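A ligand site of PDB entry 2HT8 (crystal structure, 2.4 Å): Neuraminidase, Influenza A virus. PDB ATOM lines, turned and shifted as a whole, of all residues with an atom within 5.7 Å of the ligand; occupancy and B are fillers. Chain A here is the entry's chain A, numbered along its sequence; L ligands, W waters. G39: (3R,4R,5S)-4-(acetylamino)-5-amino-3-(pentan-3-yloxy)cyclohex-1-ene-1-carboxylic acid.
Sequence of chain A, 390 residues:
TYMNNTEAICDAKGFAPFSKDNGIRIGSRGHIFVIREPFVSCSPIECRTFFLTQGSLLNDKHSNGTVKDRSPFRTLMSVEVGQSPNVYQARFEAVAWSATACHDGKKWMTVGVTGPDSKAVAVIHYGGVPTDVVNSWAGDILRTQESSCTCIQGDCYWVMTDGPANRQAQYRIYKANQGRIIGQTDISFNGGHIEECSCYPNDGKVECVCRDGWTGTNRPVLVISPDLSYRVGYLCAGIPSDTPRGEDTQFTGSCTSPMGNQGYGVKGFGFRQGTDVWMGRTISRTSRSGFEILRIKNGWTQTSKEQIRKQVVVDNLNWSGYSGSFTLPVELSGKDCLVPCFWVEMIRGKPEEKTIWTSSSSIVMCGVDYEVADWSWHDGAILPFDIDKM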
ATOM      1  N   ARG A  36      -3.166  19.355 -15.332  1.00  0.00           N
ATOM      2  CA  ARG A  36      -3.223  18.127 -16.110  1.00  0.00           C
ATOM      3  C   ARG A  36      -2.638  18.429 -17.498  1.00  0.00           C
ATOM      4  O   ARG A  36      -2.495  19.592 -17.866  1.00  0.00           O
ATOM      5  CB  ARG A  36      -4.664  17.651 -16.213  1.00  0.00           C
ATOM      6  CG  ARG A  36      -4.863  16.420 -17.060  1.00  0.00           C
ATOM      7  CD  ARG A  36      -5.015  15.169 -16.246  1.00  0.00           C
ATOM      8  NE  ARG A  36      -4.737  14.048 -17.129  1.00  0.00           N
ATOM      9  CZ  ARG A  36      -5.521  13.676 -18.134  1.00  0.00           C
ATOM     10  NH1 ARG A  36      -5.184  12.664 -18.900  1.00  0.00           N
ATOM     11  NH2 ARG A  36      -6.669  14.299 -18.335  1.00  0.00           N
ATOM     12  N   GLU A  37      -2.331  17.388 -18.264  1.00  0.00           N
ATOM     13  CA  GLU A  37      -1.733  17.529 -19.602  1.00  0.00           C
ATOM     14  C   GLU A  37      -0.454  18.350 -19.529  1.00  0.00           C
ATOM     15  O   GLU A  37      -0.318  19.387 -20.168  1.00  0.00           O
ATOM     16  CB  GLU A  37      -2.688  18.212 -20.593  1.00  0.00           C
ATOM     17  CG  GLU A  37      -3.955  17.434 -20.875  1.00  0.00           C
ATOM     18  CD  GLU A  37      -5.054  17.771 -19.900  1.00  0.00           C
ATOM     19  OE1 GLU A  37      -5.991  16.953 -19.777  1.00  0.00           O
ATOM     20  OE2 GLU A  37      -5.001  18.839 -19.270  1.00  0.00           O
ATOM     21  N   ASP A  69     -12.287  18.424 -18.122  1.00  0.00           N
ATOM     22  CA  ASP A  69     -11.542  18.608 -19.379  1.00  0.00           C
ATOM     23  C   ASP A  69     -11.441  20.015 -19.920  1.00  0.00           C
ATOM     24  O   ASP A  69     -10.371  20.610 -19.904  1.00  0.00           O
ATOM     25  CB  ASP A  69     -12.113  17.718 -20.486  1.00  0.00           C
ATOM     26  CG  ASP A  69     -11.449  16.379 -20.560  1.00  0.00           C
ATOM     27  OD1 ASP A  69     -10.243  16.341 -20.859  1.00  0.00           O
ATOM     28  OD2 ASP A  69     -12.133  15.351 -20.321  1.00  0.00           O
ATOM     29  N   ARG A  70     -12.546  20.526 -20.440  1.00  0.00           N
ATOM     30  CA  ARG A  70     -12.545  21.865 -21.011  1.00  0.00           C
ATOM     31  C   ARG A  70     -13.398  22.809 -20.167  1.00  0.00           C
ATOM     32  O   ARG A  70     -14.416  22.419 -19.598  1.00  0.00           O
ATOM     33  CB  ARG A  70     -13.066  21.807 -22.451  1.00  0.00           C
ATOM     34  CG  ARG A  70     -12.215  20.949 -23.374  1.00  0.00           C
ATOM     35  CD  ARG A  70     -12.730  20.895 -24.820  1.00  0.00           C
ATOM     36  NE  ARG A  70     -14.086  20.328 -24.945  1.00  0.00           N
ATOM     37  CZ  ARG A  70     -14.413  19.062 -24.666  1.00  0.00           C
ATOM     38  NH1 ARG A  70     -15.671  18.676 -24.823  1.00  0.00           N
ATOM     39  NH2 ARG A  70     -13.514  18.185 -24.228  1.00  0.00           N
ATOM     40  N   ARG A  74      -9.223  27.167 -17.456  1.00  0.00           N
ATOM     41  CA  ARG A  74      -7.938  26.593 -17.834  1.00  0.00           C
ATOM     42  C   ARG A  74      -7.123  27.543 -18.695  1.00  0.00           C
ATOM     43  O   ARG A  74      -7.610  28.050 -19.698  1.00  0.00           O
ATOM     44  CB  ARG A  74      -8.117  25.304 -18.647  1.00  0.00           C
ATOM     45  CG  ARG A  74      -9.014  24.237 -18.037  1.00  0.00           C
ATOM     46  CD  ARG A  74      -8.709  22.859 -18.633  1.00  0.00           C
ATOM     47  NE  ARG A  74      -7.492  22.293 -18.059  1.00  0.00           N
ATOM     48  CZ  ARG A  74      -7.003  21.087 -18.362  1.00  0.00           C
ATOM     49  NH1 ARG A  74      -5.888  20.654 -17.776  1.00  0.00           N
ATOM     50  NH2 ARG A  74      -7.624  20.326 -19.255  1.00  0.00           N
ATOM     51  N   TRP A  97      -7.378  25.191 -22.906  1.00  0.00           N
ATOM     52  CA  TRP A  97      -7.833  23.960 -22.297  1.00  0.00           C
ATOM     53  C   TRP A  97      -7.252  22.884 -23.199  1.00  0.00           C
ATOM     54  O   TRP A  97      -7.732  21.757 -23.229  1.00  0.00           O
ATOM     55  CB  TRP A  97      -9.361  23.877 -22.206  1.00  0.00           C
ATOM     56  CG  TRP A  97     -10.195  24.338 -23.402  1.00  0.00           C
ATOM     57  CD1 TRP A  97     -11.217  25.240 -23.359  1.00  0.00           C
ATOM     58  CD2 TRP A  97     -10.162  23.862 -24.757  1.00  0.00           C
ATOM     59  NE1 TRP A  97     -11.826  25.347 -24.588  1.00  0.00           N
ATOM     60  CE2 TRP A  97     -11.191  24.509 -25.461  1.00  0.00           C
ATOM     61  CE3 TRP A  97      -9.354  22.935 -25.440  1.00  0.00           C
ATOM     62  CZ2 TRP A  97     -11.444  24.275 -26.813  1.00  0.00           C
ATOM     63  CZ3 TRP A  97      -9.602  22.710 -26.782  1.00  0.00           C
ATOM     64  CH2 TRP A  97     -10.641  23.369 -27.460  1.00  0.00           C
ATOM     65  N   SER A  98      -6.224  23.282 -23.935  1.00  0.00           N
ATOM     66  CA  SER A  98      -5.483  22.434 -24.873  1.00  0.00           C
ATOM     67  C   SER A  98      -4.397  23.337 -25.498  1.00  0.00           C
ATOM     68  O   SER A  98      -4.706  24.300 -26.202  1.00  0.00           O
ATOM     69  CB  SER A  98      -6.426  21.869 -25.928  1.00  0.00           C
ATOM     70  OG  SER A  98      -5.764  20.979 -26.817  1.00  0.00           O
ATOM     71  N   ILE A 141     -14.492  20.653 -31.425  1.00  0.00           N
ATOM     72  CA  ILE A 141     -13.359  20.712 -30.533  1.00  0.00           C
ATOM     73  C   ILE A 141     -12.015  20.899 -31.243  1.00  0.00           C
ATOM     74  O   ILE A 141     -11.367  19.929 -31.609  1.00  0.00           O
ATOM     75  CB  ILE A 141     -13.256  19.447 -29.650  1.00  0.00           C
ATOM     76  CG1 ILE A 141     -14.548  19.278 -28.848  1.00  0.00           C
ATOM     77  CG2 ILE A 141     -12.018  19.555 -28.732  1.00  0.00           C
ATOM     78  CD1 ILE A 141     -14.474  18.182 -27.799  1.00  0.00           C
ATOM     79  N   ARG A 143      -8.609  20.972 -31.043  1.00  0.00           N
ATOM     80  CA  ARG A 143      -7.592  20.597 -30.070  1.00  0.00           C
ATOM     81  C   ARG A 143      -6.218  20.347 -30.721  1.00  0.00           C
ATOM     82  O   ARG A 143      -6.134  20.139 -31.928  1.00  0.00           O
ATOM     83  CB  ARG A 143      -8.053  19.344 -29.314  1.00  0.00           C
ATOM     84  CG  ARG A 143      -8.563  18.215 -30.210  1.00  0.00           C
ATOM     85  CD  ARG A 143      -9.323  17.153 -29.398  1.00  0.00           C
ATOM     86  NE  ARG A 143      -9.754  16.020 -30.217  1.00  0.00           N
ATOM     87  CZ  ARG A 143     -10.660  16.091 -31.190  1.00  0.00           C
ATOM     88  NH1 ARG A 143     -10.975  15.002 -31.884  1.00  0.00           N
ATOM     89  NH2 ARG A 143     -11.271  17.239 -31.450  1.00  0.00           N
ATOM     90  N   GLU A 146      -0.670  19.003 -26.769  1.00  0.00           N
ATOM     91  CA  GLU A 146      -0.482  18.739 -25.335  1.00  0.00           C
ATOM     92  C   GLU A 146       0.948  18.223 -25.202  1.00  0.00           C
ATOM     93  O   GLU A 146       1.276  17.499 -24.277  1.00  0.00           O
ATOM     94  CB  GLU A 146      -1.454  17.661 -24.821  1.00  0.00           C
ATOM     95  CG  GLU A 146      -2.915  17.805 -25.242  1.00  0.00           C
ATOM     96  CD  GLU A 146      -3.513  19.165 -24.892  1.00  0.00           C
ATOM     97  OE1 GLU A 146      -2.950  19.868 -24.028  1.00  0.00           O
ATOM     98  OE2 GLU A 146      -4.566  19.515 -25.473  1.00  0.00           O
ATOM     99  N   ALA A 165     -13.778  12.625 -31.450  1.00  0.00           N
ATOM    100  CA  ALA A 165     -12.683  11.887 -30.817  1.00  0.00           C
ATOM    101  C   ALA A 165     -12.767  10.393 -31.140  1.00  0.00           C
ATOM    102  O   ALA A 165     -11.774   9.664 -31.030  1.00  0.00           O
ATOM    103  CB  ALA A 165     -12.723  12.083 -29.313  1.00  0.00           C
ATOM    104  N   GLU A 195      -4.293  12.218 -32.818  1.00  0.00           N
ATOM    105  CA  GLU A 195      -4.611  13.055 -31.654  1.00  0.00           C
ATOM    106  C   GLU A 195      -3.390  13.245 -30.772  1.00  0.00           C
ATOM    107  O   GLU A 195      -2.569  12.342 -30.640  1.00  0.00           O
ATOM    108  CB  GLU A 195      -5.689  12.408 -30.796  1.00  0.00           C
ATOM    109  CG  GLU A 195      -7.030  12.243 -31.454  1.00  0.00           C
ATOM    110  CD  GLU A 195      -7.963  13.392 -31.160  1.00  0.00           C
ATOM    111  OE1 GLU A 195      -9.158  13.267 -31.466  1.00  0.00           O
ATOM    112  OE2 GLU A 195      -7.493  14.421 -30.613  1.00  0.00           O
ATOM    113  N   GLU A 196      -3.296  14.424 -30.164  1.00  0.00           N
ATOM    114  CA  GLU A 196      -2.203  14.723 -29.247  1.00  0.00           C
ATOM    115  C   GLU A 196      -0.904  14.068 -29.700  1.00  0.00           C
ATOM    116  O   GLU A 196      -0.438  13.125 -29.054  1.00  0.00           O
ATOM    117  CB  GLU A 196      -2.563  14.195 -27.856  1.00  0.00           C
ATOM    118  CG  GLU A 196      -4.025  14.387 -27.447  1.00  0.00           C
ATOM    119  CD  GLU A 196      -4.445  13.479 -26.300  1.00  0.00           C
ATOM    120  OE1 GLU A 196      -4.192  12.256 -26.366  1.00  0.00           O
ATOM    121  OE2 GLU A 196      -5.051  13.976 -25.333  1.00  0.00           O
ATOM    122  N   ARG A 211      -1.834   9.728 -31.524  1.00  0.00           N
ATOM    123  CA  ARG A 211      -2.786   8.860 -30.834  1.00  0.00           C
ATOM    124  C   ARG A 211      -4.034   8.560 -31.651  1.00  0.00           C
ATOM    125  O   ARG A 211      -4.834   9.454 -31.918  1.00  0.00           O
ATOM    126  CB  ARG A 211      -3.197   9.474 -29.487  1.00  0.00           C
ATOM    127  CG  ARG A 211      -4.452   8.865 -28.833  1.00  0.00           C
ATOM    128  CD  ARG A 211      -4.878   9.659 -27.604  1.00  0.00           C
ATOM    129  NE  ARG A 211      -6.160   9.248 -27.025  1.00  0.00           N
ATOM    130  CZ  ARG A 211      -6.678   9.788 -25.916  1.00  0.00           C
ATOM    131  NH1 ARG A 211      -7.860   9.369 -25.453  1.00  0.00           N
ATOM    132  NH2 ARG A 211      -6.013  10.744 -25.257  1.00  0.00           N
ATOM    133  N   TYR A 264     -10.266   3.432 -27.547  1.00  0.00           N
ATOM    134  CA  TYR A 264      -9.864   4.605 -26.782  1.00  0.00           C
ATOM    135  C   TYR A 264      -8.363   4.812 -26.881  1.00  0.00           C
ATOM    136  O   TYR A 264      -7.752   4.598 -27.938  1.00  0.00           O
ATOM    137  CB  TYR A 264     -10.280   4.447 -25.314  1.00  0.00           C
ATOM    138  CG  TYR A 264     -10.353   5.769 -24.557  1.00  0.00           C
ATOM    139  CD1 TYR A 264     -11.157   6.805 -25.027  1.00  0.00           C
ATOM    140  CD2 TYR A 264      -9.610   5.978 -23.390  1.00  0.00           C
ATOM    141  CE1 TYR A 264     -11.219   8.027 -24.358  1.00  0.00           C
ATOM    142  CE2 TYR A 264      -9.671   7.196 -22.708  1.00  0.00           C
ATOM    143  CZ  TYR A 264     -10.478   8.218 -23.203  1.00  0.00           C
ATOM    144  OH  TYR A 264     -10.566   9.431 -22.565  1.00  0.00           O
ATOM    145  N   GLY A 265      -7.763   5.253 -25.784  1.00  0.00           N
ATOM    146  CA  GLY A 265      -6.335   5.477 -25.780  1.00  0.00           C
ATOM    147  C   GLY A 265      -5.896   6.520 -24.788  1.00  0.00           C
ATOM    148  O   GLY A 265      -6.683   7.010 -23.979  1.00  0.00           O
ATOM    149  N   VAL A 266      -4.609   6.833 -24.836  1.00  0.00           N
ATOM    150  CA  VAL A 266      -3.989   7.834 -24.001  1.00  0.00           C
ATOM    151  C   VAL A 266      -2.838   8.413 -24.822  1.00  0.00           C
ATOM    152  O   VAL A 266      -2.413   7.817 -25.811  1.00  0.00           O
ATOM    153  CB  VAL A 266      -3.468   7.236 -22.693  1.00  0.00           C
ATOM    154  CG1 VAL A 266      -2.259   6.370 -22.968  1.00  0.00           C
ATOM    155  CG2 VAL A 266      -3.151   8.340 -21.717  1.00  0.00           C
ATOM    156  N   ARG A 288      -4.638   3.163 -16.468  1.00  0.00           N
ATOM    157  CA  ARG A 288      -3.522   4.092 -16.609  1.00  0.00           C
ATOM    158  C   ARG A 288      -2.591   3.972 -15.408  1.00  0.00           C
ATOM    159  O   ARG A 288      -2.456   4.875 -14.585  1.00  0.00           O
ATOM    160  CB  ARG A 288      -4.043   5.509 -16.804  1.00  0.00           C
ATOM    161  CG  ARG A 288      -4.507   5.743 -18.245  1.00  0.00           C
ATOM    162  CD  ARG A 288      -5.184   7.082 -18.442  1.00  0.00           C
ATOM    163  NE  ARG A 288      -5.424   7.380 -19.850  1.00  0.00           N
ATOM    164  CZ  ARG A 288      -5.947   8.518 -20.300  1.00  0.00           C
ATOM    165  NH1 ARG A 288      -6.126   8.693 -21.604  1.00  0.00           N
ATOM    166  NH2 ARG A 288      -6.283   9.485 -19.451  1.00  0.00           N
ATOM    167  N   TYR A 322      -0.231  10.319 -19.385  1.00  0.00           N
ATOM    168  CA  TYR A 322       0.335  10.911 -20.611  1.00  0.00           C
ATOM    169  C   TYR A 322       1.861  10.813 -20.708  1.00  0.00           C
ATOM    170  O   TYR A 322       2.558  10.702 -19.725  1.00  0.00           O
ATOM    171  CB  TYR A 322      -0.098  12.378 -20.721  1.00  0.00           C
ATOM    172  CG  TYR A 322      -1.462  12.565 -21.323  1.00  0.00           C
ATOM    173  CD1 TYR A 322      -2.500  11.661 -21.060  1.00  0.00           C
ATOM    174  CD2 TYR A 322      -1.713  13.592 -22.239  1.00  0.00           C
ATOM    175  CE1 TYR A 322      -3.730  11.770 -21.689  1.00  0.00           C
ATOM    176  CE2 TYR A 322      -2.945  13.710 -22.865  1.00  0.00           C
ATOM    177  CZ  TYR A 322      -3.942  12.780 -22.588  1.00  0.00           C
ATOM    178  OH  TYR A 322      -5.150  12.831 -23.256  1.00  0.00           O
ATOM    179  N   ILE A 347      -1.352  10.931 -13.174  1.00  0.00           N
ATOM    180  CA  ILE A 347      -2.653  11.440 -12.769  1.00  0.00           C
ATOM    181  C   ILE A 347      -3.127  10.788 -11.482  1.00  0.00           C
ATOM    182  O   ILE A 347      -2.992   9.572 -11.300  1.00  0.00           O
ATOM    183  CB  ILE A 347      -3.711  11.204 -13.875  1.00  0.00           C
ATOM    184  CG1 ILE A 347      -3.263  11.848 -15.192  1.00  0.00           C
ATOM    185  CG2 ILE A 347      -5.054  11.804 -13.451  1.00  0.00           C
ATOM    186  CD1 ILE A 347      -4.100  11.411 -16.347  1.00  0.00           C
HETATM  187  C1  G39 L   1      -7.945  11.708 -21.838  1.00  0.00           C
HETATM  188  O1A G39 L   1      -8.053  10.665 -22.525  1.00  0.00           O
HETATM  189  O1B G39 L   1      -7.658  11.648 -20.622  1.00  0.00           O
HETATM  190  C2  G39 L   1      -8.111  12.969 -22.499  1.00  0.00           C
HETATM  191  C3  G39 L   1      -7.857  14.352 -21.729  1.00  0.00           C
HETATM  192  C4  G39 L   1      -7.716  15.656 -22.586  1.00  0.00           C
HETATM  193  C5  G39 L   1      -8.784  15.625 -23.671  1.00  0.00           C
HETATM  194  N5  G39 L   1      -8.663  16.860 -24.526  1.00  0.00           N
HETATM  195  C10 G39 L   1      -9.664  17.764 -24.475  1.00  0.00           C
HETATM  196  O10 G39 L   1     -10.683  17.648 -23.748  1.00  0.00           O
HETATM  197  C11 G39 L   1      -9.546  18.977 -25.328  1.00  0.00           C
HETATM  198  C6  G39 L   1      -8.605  14.335 -24.562  1.00  0.00           C
HETATM  199  C7  G39 L   1      -8.465  13.024 -23.862  1.00  0.00           C
HETATM  200  O7  G39 L   1      -9.708  14.347 -25.567  1.00  0.00           O
HETATM  201  C8  G39 L   1      -9.575  14.700 -26.978  1.00  0.00           C
HETATM  202  C9  G39 L   1      -8.590  13.843 -27.795  1.00  0.00           C
HETATM  203  C81 G39 L   1     -10.982  14.584 -27.525  1.00  0.00           C
HETATM  204  C82 G39 L   1     -11.806  15.795 -27.210  1.00  0.00           C
HETATM  205  C91 G39 L   1      -8.921  12.345 -27.823  1.00  0.00           C
HETATM  206  N4  G39 L   1      -7.899  16.772 -21.686  1.00  0.00           N
HETATM  207  O   HOH W   1      -6.508  19.164 -23.680  1.00  0.00           O
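The side-chain carboxylate (OD1) of Asp 69 lies within salt-bridge range of a nitrogen (N4) of the ligand. A nitrogen (N4) of the ligand is in salt-bridge range of the side-chain carboxylate of Glu 37. The side-chain hydroxyl of Tyr 264 sits at hydrogen-bond distance from an oxygen (O1A) of the ligand (2.8 Å). NH2 of Arg 288 lies within salt-bridge range of O1B of the ligand (2.8 Å). The guanidinium group (NH2) of Arg 70 lies within hydrogen-bond range of an oxygen (O10) of the ligand (2.9 Å). The guanidinium group (NH1) of Arg 36 lies within salt-bridge range of an oxygen (O1B) of the ligand (3.2 Å). An oxygen (O1A) of the ligand is in salt-bridge range of the guanidinium group (NH1) of Arg 211, at 3.2 Å.
O of Asp 69 is in hydrogen-bond range of NH2 of Arg 74 (2.8 Å). OE1 of Glu 37 is in salt-bridge range of NH2 of Arg 36 (3.1 Å). The side-chain carboxylate of Glu 37 is in salt-bridge range of the guanidinium group of Arg 74 (2.5 Å). NH1 of Arg 288 is in hydrogen-bond range of O of Gly 265 (3.0 Å). O of Glu 195 is in hydrogen-bond range of N of Arg 211 (2.9 Å). NH2 of Arg 211 lies within salt-bridge range of OE1 of Glu 196, at 2.6 Å. NH1 of Arg 211 lies within hydrogen-bond range of O of Gly 265 (3.0 Å). NH2 of Arg 143 is in hydrogen-bond range of O of Ile 141, 2.7 Å away.
Merely in contact with the ligand: Trp 97, Ile 141, Arg 143, Ala 165, Glu 195, Glu 196 and Tyr 322. Hydrophobic or aromatic side chains that line the ligand: Trp 97, Ile 141, Ala 165 and Tyr 264. 14 residues have an atom within 4 Å of the ligand: Arg 36, Glu 37, Asp 69, Arg 70, Trp 97, Ile 141, Arg 143, Ala 165, Glu 195, Glu 196, Arg 211, Tyr 264, Arg 288 and Tyr 322.
Water W1 lies within hydrogen-bond range of OE2 of Glu 146 (2.7 Å), O of Trp 97 (2.9 Å) and N5 of the ligand (3.3 Å).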
